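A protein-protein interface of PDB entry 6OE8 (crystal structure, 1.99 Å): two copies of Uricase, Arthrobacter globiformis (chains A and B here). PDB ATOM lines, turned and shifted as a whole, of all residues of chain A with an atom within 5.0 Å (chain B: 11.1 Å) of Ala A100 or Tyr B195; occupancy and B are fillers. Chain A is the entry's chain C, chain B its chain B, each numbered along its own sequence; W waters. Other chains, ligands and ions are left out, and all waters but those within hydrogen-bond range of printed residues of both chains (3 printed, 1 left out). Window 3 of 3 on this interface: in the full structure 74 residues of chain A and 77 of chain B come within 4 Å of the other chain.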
ATOM      1  N   THR A  93     -23.698  17.274 -29.080  1.00  0.00           N
ATOM      2  CA  THR A  93     -24.404  18.082 -28.091  1.00  0.00           C
ATOM      3  C   THR A  93     -24.616  17.305 -26.794  1.00  0.00           C
ATOM      4  O   THR A  93     -24.500  17.872 -25.700  1.00  0.00           O
ATOM      5  CB  THR A  93     -25.737  18.577 -28.667  1.00  0.00           C
ATOM      6  OG1 THR A  93     -25.488  19.388 -29.825  1.00  0.00           O
ATOM      7  CG2 THR A  93     -26.494  19.393 -27.641  1.00  0.00           C
ATOM      8  N   ASN A  96     -21.350  17.459 -24.961  1.00  0.00           N
ATOM      9  CA  ASN A  96     -21.146  18.773 -24.369  1.00  0.00           C
ATOM     10  C   ASN A  96     -21.998  18.936 -23.124  1.00  0.00           C
ATOM     11  O   ASN A  96     -21.567  19.545 -22.137  1.00  0.00           O
ATOM     12  CB  ASN A  96     -21.501  19.877 -25.359  1.00  0.00           C
ATOM     13  CG  ASN A  96     -20.552  19.947 -26.526  1.00  0.00           C
ATOM     14  OD1 ASN A  96     -19.362  19.671 -26.398  1.00  0.00           O
ATOM     15  ND2 ASN A  96     -21.064  20.413 -27.658  1.00  0.00           N
ATOM     16  N   THR A  97     -23.219  18.399 -23.160  1.00  0.00           N
ATOM     17  CA  THR A  97     -24.104  18.505 -22.010  1.00  0.00           C
ATOM     18  C   THR A  97     -23.509  17.774 -20.818  1.00  0.00           C
ATOM     19  O   THR A  97     -23.579  18.256 -19.681  1.00  0.00           O
ATOM     20  CB  THR A  97     -25.480  17.943 -22.359  1.00  0.00           C
ATOM     21  OG1 THR A  97     -26.004  18.641 -23.495  1.00  0.00           O
ATOM     22  CG2 THR A  97     -26.438  18.122 -21.189  1.00  0.00           C
ATOM     23  N   VAL A  98     -22.892  16.615 -21.068  1.00  0.00           N
ATOM     24  CA  VAL A  98     -22.226  15.894 -19.982  1.00  0.00           C
ATOM     25  C   VAL A  98     -21.205  16.791 -19.292  1.00  0.00           C
ATOM     26  O   VAL A  98     -21.224  16.954 -18.063  1.00  0.00           O
ATOM     27  CB  VAL A  98     -21.573  14.603 -20.506  1.00  0.00           C
ATOM     28  CG1 VAL A  98     -20.694  13.971 -19.423  1.00  0.00           C
ATOM     29  CG2 VAL A  98     -22.645  13.620 -20.957  1.00  0.00           C
ATOM     30  N   TYR A  99     -20.310  17.412 -20.072  1.00  0.00           N
ATOM     31  CA  TYR A  99     -19.249  18.191 -19.414  1.00  0.00           C
ATOM     32  C   TYR A  99     -19.787  19.463 -18.749  1.00  0.00           C
ATOM     33  O   TYR A  99     -19.371  19.822 -17.624  1.00  0.00           O
ATOM     34  CB  TYR A  99     -18.128  18.523 -20.400  1.00  0.00           C
ATOM     35  CG  TYR A  99     -17.337  17.309 -20.834  1.00  0.00           C
ATOM     36  CD1 TYR A  99     -16.399  16.728 -19.984  1.00  0.00           C
ATOM     37  CD2 TYR A  99     -17.521  16.747 -22.095  1.00  0.00           C
ATOM     38  CE1 TYR A  99     -15.673  15.610 -20.378  1.00  0.00           C
ATOM     39  CE2 TYR A  99     -16.798  15.629 -22.499  1.00  0.00           C
ATOM     40  CZ  TYR A  99     -15.875  15.070 -21.637  1.00  0.00           C
ATOM     41  OH  TYR A  99     -15.153  13.966 -22.034  1.00  0.00           O
ATOM     42  N   ALA A 100     -20.762  20.120 -19.390  1.00  0.00           N
ATOM     43  CA  ALA A 100     -21.331  21.339 -18.826  1.00  0.00           C
ATOM     44  C   ALA A 100     -22.040  21.048 -17.511  1.00  0.00           C
ATOM     45  O   ALA A 100     -21.901  21.800 -16.541  1.00  0.00           O
ATOM     46  CB  ALA A 100     -22.286  21.988 -19.832  1.00  0.00           C
ATOM     47  N   PHE A 101     -22.829  19.975 -17.468  1.00  0.00           N
ATOM     48  CA  PHE A 101     -23.482  19.578 -16.226  1.00  0.00           C
ATOM     49  C   PHE A 101     -22.454  19.201 -15.161  1.00  0.00           C
ATOM     50  O   PHE A 101     -22.639  19.508 -13.978  1.00  0.00           O
ATOM     51  CB  PHE A 101     -24.435  18.426 -16.545  1.00  0.00           C
ATOM     52  CG  PHE A 101     -25.789  18.879 -17.038  1.00  0.00           C
ATOM     53  CD1 PHE A 101     -26.939  18.545 -16.371  1.00  0.00           C
ATOM     54  CD2 PHE A 101     -25.887  19.768 -18.098  1.00  0.00           C
ATOM     55  CE1 PHE A 101     -28.176  18.996 -16.819  1.00  0.00           C
ATOM     56  CE2 PHE A 101     -27.122  20.239 -18.536  1.00  0.00           C
ATOM     57  CZ  PHE A 101     -28.259  19.849 -17.894  1.00  0.00           C
ATOM     58  N   ALA A 102     -21.341  18.563 -15.566  1.00  0.00           N
ATOM     59  CA  ALA A 102     -20.327  18.187 -14.586  1.00  0.00           C
ATOM     60  C   ALA A 102     -19.760  19.404 -13.873  1.00  0.00           C
ATOM     61  O   ALA A 102     -19.306  19.294 -12.728  1.00  0.00           O
ATOM     62  CB  ALA A 102     -19.199  17.394 -15.250  1.00  0.00           C
ATOM     63  N   ARG A 103     -19.727  20.556 -14.550  1.00  0.00           N
ATOM     64  CA  ARG A 103     -19.174  21.755 -13.910  1.00  0.00           C
ATOM     65  C   ARG A 103     -19.858  22.081 -12.582  1.00  0.00           C
ATOM     66  O   ARG A 103     -19.204  22.540 -11.639  1.00  0.00           O
ATOM     67  CB  ARG A 103     -19.280  22.953 -14.853  1.00  0.00           C
ATOM     68  CG  ARG A 103     -18.905  24.303 -14.236  1.00  0.00           C
ATOM     69  CD  ARG A 103     -17.455  24.425 -13.824  1.00  0.00           C
ATOM     70  NE  ARG A 103     -17.178  25.754 -13.266  1.00  0.00           N
ATOM     71  CZ  ARG A 103     -17.320  26.088 -11.985  1.00  0.00           C
ATOM     72  NH1 ARG A 103     -17.731  25.192 -11.100  1.00  0.00           N
ATOM     73  NH2 ARG A 103     -17.039  27.319 -11.583  1.00  0.00           N
ATOM     74  N   ASP A 104     -21.172  21.860 -12.490  1.00  0.00           N
ATOM     75  CA  ASP A 104     -21.923  22.122 -11.265  1.00  0.00           C
ATOM     76  C   ASP A 104     -21.638  21.122 -10.148  1.00  0.00           C
ATOM     77  O   ASP A 104     -22.050  21.362  -9.007  1.00  0.00           O
ATOM     78  CB  ASP A 104     -23.415  22.102 -11.585  1.00  0.00           C
ATOM     79  CG  ASP A 104     -23.814  23.193 -12.557  1.00  0.00           C
ATOM     80  OD1 ASP A 104     -23.177  24.269 -12.562  1.00  0.00           O
ATOM     81  OD2 ASP A 104     -24.750  22.959 -13.342  1.00  0.00           O
ATOM     82  N   HIS A 119     -32.987  16.241 -18.075  1.00  0.00           N
ATOM     83  CA  HIS A 119     -32.727  17.327 -19.012  1.00  0.00           C
ATOM     84  C   HIS A 119     -33.210  16.968 -20.409  1.00  0.00           C
ATOM     85  O   HIS A 119     -33.934  17.742 -21.048  1.00  0.00           O
ATOM     86  CB  HIS A 119     -31.237  17.663 -19.065  1.00  0.00           C
ATOM     87  CG  HIS A 119     -30.896  18.658 -20.129  1.00  0.00           C
ATOM     88  ND1 HIS A 119     -31.162  20.005 -20.003  1.00  0.00           N
ATOM     89  CD2 HIS A 119     -30.368  18.494 -21.365  1.00  0.00           C
ATOM     90  CE1 HIS A 119     -30.779  20.632 -21.101  1.00  0.00           C
ATOM     91  NE2 HIS A 119     -30.298  19.737 -21.947  1.00  0.00           N
ATOM     92  N   PHE B 190     -29.750  19.800 -37.807  1.00  0.00           N
ATOM     93  CA  PHE B 190     -30.018  19.379 -36.445  1.00  0.00           C
ATOM     94  C   PHE B 190     -30.295  20.591 -35.556  1.00  0.00           C
ATOM     95  O   PHE B 190     -29.787  21.684 -35.807  1.00  0.00           O
ATOM     96  CB  PHE B 190     -28.848  18.554 -35.899  1.00  0.00           C
ATOM     97  CG  PHE B 190     -27.506  19.245 -35.971  1.00  0.00           C
ATOM     98  CD1 PHE B 190     -26.717  19.129 -37.108  1.00  0.00           C
ATOM     99  CD2 PHE B 190     -27.013  19.967 -34.895  1.00  0.00           C
ATOM    100  CE1 PHE B 190     -25.474  19.745 -37.185  1.00  0.00           C
ATOM    101  CE2 PHE B 190     -25.771  20.585 -34.964  1.00  0.00           C
ATOM    102  CZ  PHE B 190     -25.002  20.475 -36.110  1.00  0.00           C
ATOM    103  N   PRO B 191     -31.097  20.423 -34.510  1.00  0.00           N
ATOM    104  CA  PRO B 191     -31.461  21.578 -33.680  1.00  0.00           C
ATOM    105  C   PRO B 191     -30.264  22.077 -32.890  1.00  0.00           C
ATOM    106  O   PRO B 191     -29.327  21.328 -32.600  1.00  0.00           O
ATOM    107  CB  PRO B 191     -32.550  21.022 -32.754  1.00  0.00           C
ATOM    108  CG  PRO B 191     -32.265  19.545 -32.692  1.00  0.00           C
ATOM    109  CD  PRO B 191     -31.748  19.180 -34.056  1.00  0.00           C
ATOM    110  N   ARG B 192     -30.288  23.367 -32.553  1.00  0.00           N
ATOM    111  CA  ARG B 192     -29.149  24.002 -31.897  1.00  0.00           C
ATOM    112  C   ARG B 192     -29.622  24.590 -30.577  1.00  0.00           C
ATOM    113  O   ARG B 192     -30.231  25.664 -30.550  1.00  0.00           O
ATOM    114  CB  ARG B 192     -28.532  25.082 -32.775  1.00  0.00           C
ATOM    115  CG  ARG B 192     -28.066  24.575 -34.120  1.00  0.00           C
ATOM    116  CD  ARG B 192     -27.312  25.636 -34.887  1.00  0.00           C
ATOM    117  NE  ARG B 192     -26.016  25.880 -34.257  1.00  0.00           N
ATOM    118  CZ  ARG B 192     -24.919  25.177 -34.527  1.00  0.00           C
ATOM    119  NH1 ARG B 192     -24.969  24.194 -35.416  1.00  0.00           N
ATOM    120  NH2 ARG B 192     -23.776  25.448 -33.912  1.00  0.00           N
ATOM    121  N   ASP B 193     -29.293  23.917 -29.484  1.00  0.00           N
ATOM    122  CA  ASP B 193     -29.654  24.356 -28.149  1.00  0.00           C
ATOM    123  C   ASP B 193     -28.464  25.059 -27.503  1.00  0.00           C
ATOM    124  O   ASP B 193     -27.433  25.309 -28.143  1.00  0.00           O
ATOM    125  CB  ASP B 193     -30.198  23.175 -27.327  1.00  0.00           C
ATOM    126  CG  ASP B 193     -29.116  22.159 -26.936  1.00  0.00           C
ATOM    127  OD1 ASP B 193     -27.960  22.293 -27.382  1.00  0.00           O
ATOM    128  OD2 ASP B 193     -29.436  21.225 -26.172  1.00  0.00           O
ATOM    129  N   LYS B 194     -28.611  25.379 -26.218  1.00  0.00           N
ATOM    130  CA  LYS B 194     -27.566  26.075 -25.483  1.00  0.00           C
ATOM    131  C   LYS B 194     -26.247  25.309 -25.486  1.00  0.00           C
ATOM    132  O   LYS B 194     -25.182  25.916 -25.336  1.00  0.00           O
ATOM    133  CB  LYS B 194     -28.041  26.281 -24.047  1.00  0.00           C
ATOM    134  CG  LYS B 194     -27.096  27.046 -23.145  1.00  0.00           C
ATOM    135  CD  LYS B 194     -27.684  27.159 -21.746  1.00  0.00           C
ATOM    136  CE  LYS B 194     -26.736  27.880 -20.798  1.00  0.00           C
ATOM    137  NZ  LYS B 194     -27.296  27.998 -19.424  1.00  0.00           N
ATOM    138  N   TYR B 195     -26.291  23.987 -25.647  1.00  0.00           N
ATOM    139  CA  TYR B 195     -25.096  23.154 -25.585  1.00  0.00           C
ATOM    140  C   TYR B 195     -24.606  22.682 -26.953  1.00  0.00           C
ATOM    141  O   TYR B 195     -23.733  21.806 -27.015  1.00  0.00           O
ATOM    142  CB  TYR B 195     -25.368  21.959 -24.668  1.00  0.00           C
ATOM    143  CG  TYR B 195     -25.824  22.383 -23.283  1.00  0.00           C
ATOM    144  CD1 TYR B 195     -24.917  22.873 -22.351  1.00  0.00           C
ATOM    145  CD2 TYR B 195     -27.168  22.323 -22.919  1.00  0.00           C
ATOM    146  CE1 TYR B 195     -25.325  23.273 -21.091  1.00  0.00           C
ATOM    147  CE2 TYR B 195     -27.588  22.722 -21.654  1.00  0.00           C
ATOM    148  CZ  TYR B 195     -26.664  23.194 -20.747  1.00  0.00           C
ATOM    149  OH  TYR B 195     -27.064  23.588 -19.490  1.00  0.00           O
ATOM    150  N   THR B 196     -25.115  23.252 -28.047  1.00  0.00           N
ATOM    151  CA  THR B 196     -24.778  22.792 -29.390  1.00  0.00           C
ATOM    152  C   THR B 196     -23.691  23.675 -29.998  1.00  0.00           C
ATOM    153  O   THR B 196     -23.893  24.878 -30.186  1.00  0.00           O
ATOM    154  CB  THR B 196     -26.012  22.771 -30.290  1.00  0.00           C
ATOM    155  OG1 THR B 196     -26.979  21.844 -29.772  1.00  0.00           O
ATOM    156  CG2 THR B 196     -25.629  22.348 -31.700  1.00  0.00           C
ATOM    157  N   THR B 197     -22.539  23.072 -30.301  1.00  0.00           N
ATOM    158  CA  THR B 197     -21.434  23.766 -30.957  1.00  0.00           C
ATOM    159  C   THR B 197     -21.008  23.147 -32.282  1.00  0.00           C
ATOM    160  O   THR B 197     -20.199  23.754 -32.995  1.00  0.00           O
ATOM    161  CB  THR B 197     -20.209  23.812 -30.032  1.00  0.00           C
ATOM    162  OG1 THR B 197     -19.838  22.473 -29.690  1.00  0.00           O
ATOM    163  CG2 THR B 197     -20.521  24.583 -28.758  1.00  0.00           C
ATOM    164  N   LEU B 198     -21.514  21.968 -32.627  1.00  0.00           N
ATOM    165  CA  LEU B 198     -21.100  21.285 -33.845  1.00  0.00           C
ATOM    166  C   LEU B 198     -21.512  22.072 -35.084  1.00  0.00           C
ATOM    167  O   LEU B 198     -22.651  22.535 -35.187  1.00  0.00           O
ATOM    168  CB  LEU B 198     -21.716  19.888 -33.886  1.00  0.00           C
ATOM    169  CG  LEU B 198     -21.345  18.994 -35.068  1.00  0.00           C
ATOM    170  CD1 LEU B 198     -19.845  18.681 -35.072  1.00  0.00           C
ATOM    171  CD2 LEU B 198     -22.173  17.716 -35.052  1.00  0.00           C
ATOM    172  N   GLN B 199     -20.587  22.209 -36.030  1.00  0.00           N
ATOM    173  CA  GLN B 199     -20.885  22.858 -37.301  1.00  0.00           C
ATOM    174  C   GLN B 199     -21.540  21.893 -38.279  1.00  0.00           C
ATOM    175  O   GLN B 199     -21.159  20.724 -38.375  1.00  0.00           O
ATOM    176  CB  GLN B 199     -19.614  23.435 -37.925  1.00  0.00           C
ATOM    177  CG  GLN B 199     -19.057  24.623 -37.177  1.00  0.00           C
ATOM    178  CD  GLN B 199     -20.008  25.808 -37.225  1.00  0.00           C
ATOM    179  OE1 GLN B 199     -20.633  26.162 -36.223  1.00  0.00           O
ATOM    180  NE2 GLN B 199     -20.126  26.425 -38.400  1.00  0.00           N
HETATM  181  O   HOH W   1     -28.578  19.243 -24.512  1.00  0.00           O
HETATM  182  O   HOH W   2     -31.285  22.278 -24.014  1.00  0.00           O
HETATM  183  O   HOH W   3     -27.970  19.329 -31.449  1.00  0.00           O
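OG1 of Thr B196 lies within hydrogen-bond range of OG1 of Thr A93. ND2 of Asn A96 is in hydrogen-bond range of OG1 of Thr B197, 3.1 Å away. O of Tyr B195 sits at hydrogen-bond distance from ND2 of Asn A96, 3.1 Å away.
Water W3 lies within hydrogen-bond range of O of Pro B191 (2.7 Å), OG1 of Thr A93 (3.0 Å) and OG1 of Thr B196 (3.2 Å). Water W1 lies within hydrogen-bond range of the side-chain carboxylate (OD2) of Asp B193 (2.7 Å), the side-chain hydroxyl (OG1) of Thr A97 (2.8 Å) and a ring nitrogen (NE2) of His A119 (3.1 Å). Water W2 lies within hydrogen-bond range of OD2 of Asp B193 and NE2 of His A119.
The side-chain carboxylate (OD1) of Asp B193 sits at hydrogen-bond distance from the backbone NH (N) of Tyr B195 (2.9 Å). The backbone carbonyl oxygen of Thr A93 is in hydrogen-bond range of the side-chain hydroxyl of Thr A97. The side-chain carboxylate (OD1) of Asp B193 sits at hydrogen-bond distance from the side-chain hydroxyl (OG1) of Thr B196 (2.6 Å).
Of chain B, only Tyr B195 (3.5 Å) comes within 4 Å of Ala A100. Tyr B195 touches just these residues of chain A: Thr A93 (3.7 Å), Asn A96 (3.1 Å), Thr A97 (3.6 Å), Ala A100 (3.5 Å), Phe A101 (3.5 Å) and His A119 (3.9 Å). Of chain B, only Asp B193, Tyr B195 and Thr B196 come within 4 Å of Thr A93. Asn A96 touches two residues of chain B. Of chain B, only Tyr B195 (3.6 Å) comes within 4 Å of Thr A97. Phe A101 touches just one residue of chain B: Tyr B195. No residue of chain B comes within 4 Å of Ala A102. Printed residues of chain A within 4 Å of Asp B193: Thr A93. Of the printed residues of chain B, His A119 touches Tyr B195 (3.9 Å). Of the printed residues of chain A, Thr B196 touches Thr A93. Of the printed residues of chain A, Thr B197 touches Asn A96. The nearest printed residue of chain A that does not touch Tyr B195 is Asp A104 (6.6 Å). The nearest printed residue of chain A that does not touch Thr B197 is Thr A93 (4.7 Å).
Of the 10 printed residues of chain B, 4 touch a printed residue of chain A. Hydrophobic or aromatic side chains of chain B within 4 Å of the printed part of chain A: Tyr B195. Hydrophobic or aromatic side chains of chain A within 4 Å of the printed part of chain B: Ala A100, Phe A101 and His A119. Among the printed residues, no Asp or Glu carboxylate lies within 4 Å of a Lys or Arg side-chain nitrogen of the other chain.
No position is printed for both chains.
OD1 of Asp B193 touches CG2 of Thr A93 (3.3 Å). Thr A93 touches Tyr B195 (CG2 to O, 3.7 Å). Tyr B195 touches Thr A97. Tyr B195 touches Ala A100. Tyr B195 touches Phe A101 (OH to CE2, 3.5 Å). CE1 of His A119 touches CE2 of Tyr B195, at 3.9 Å.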
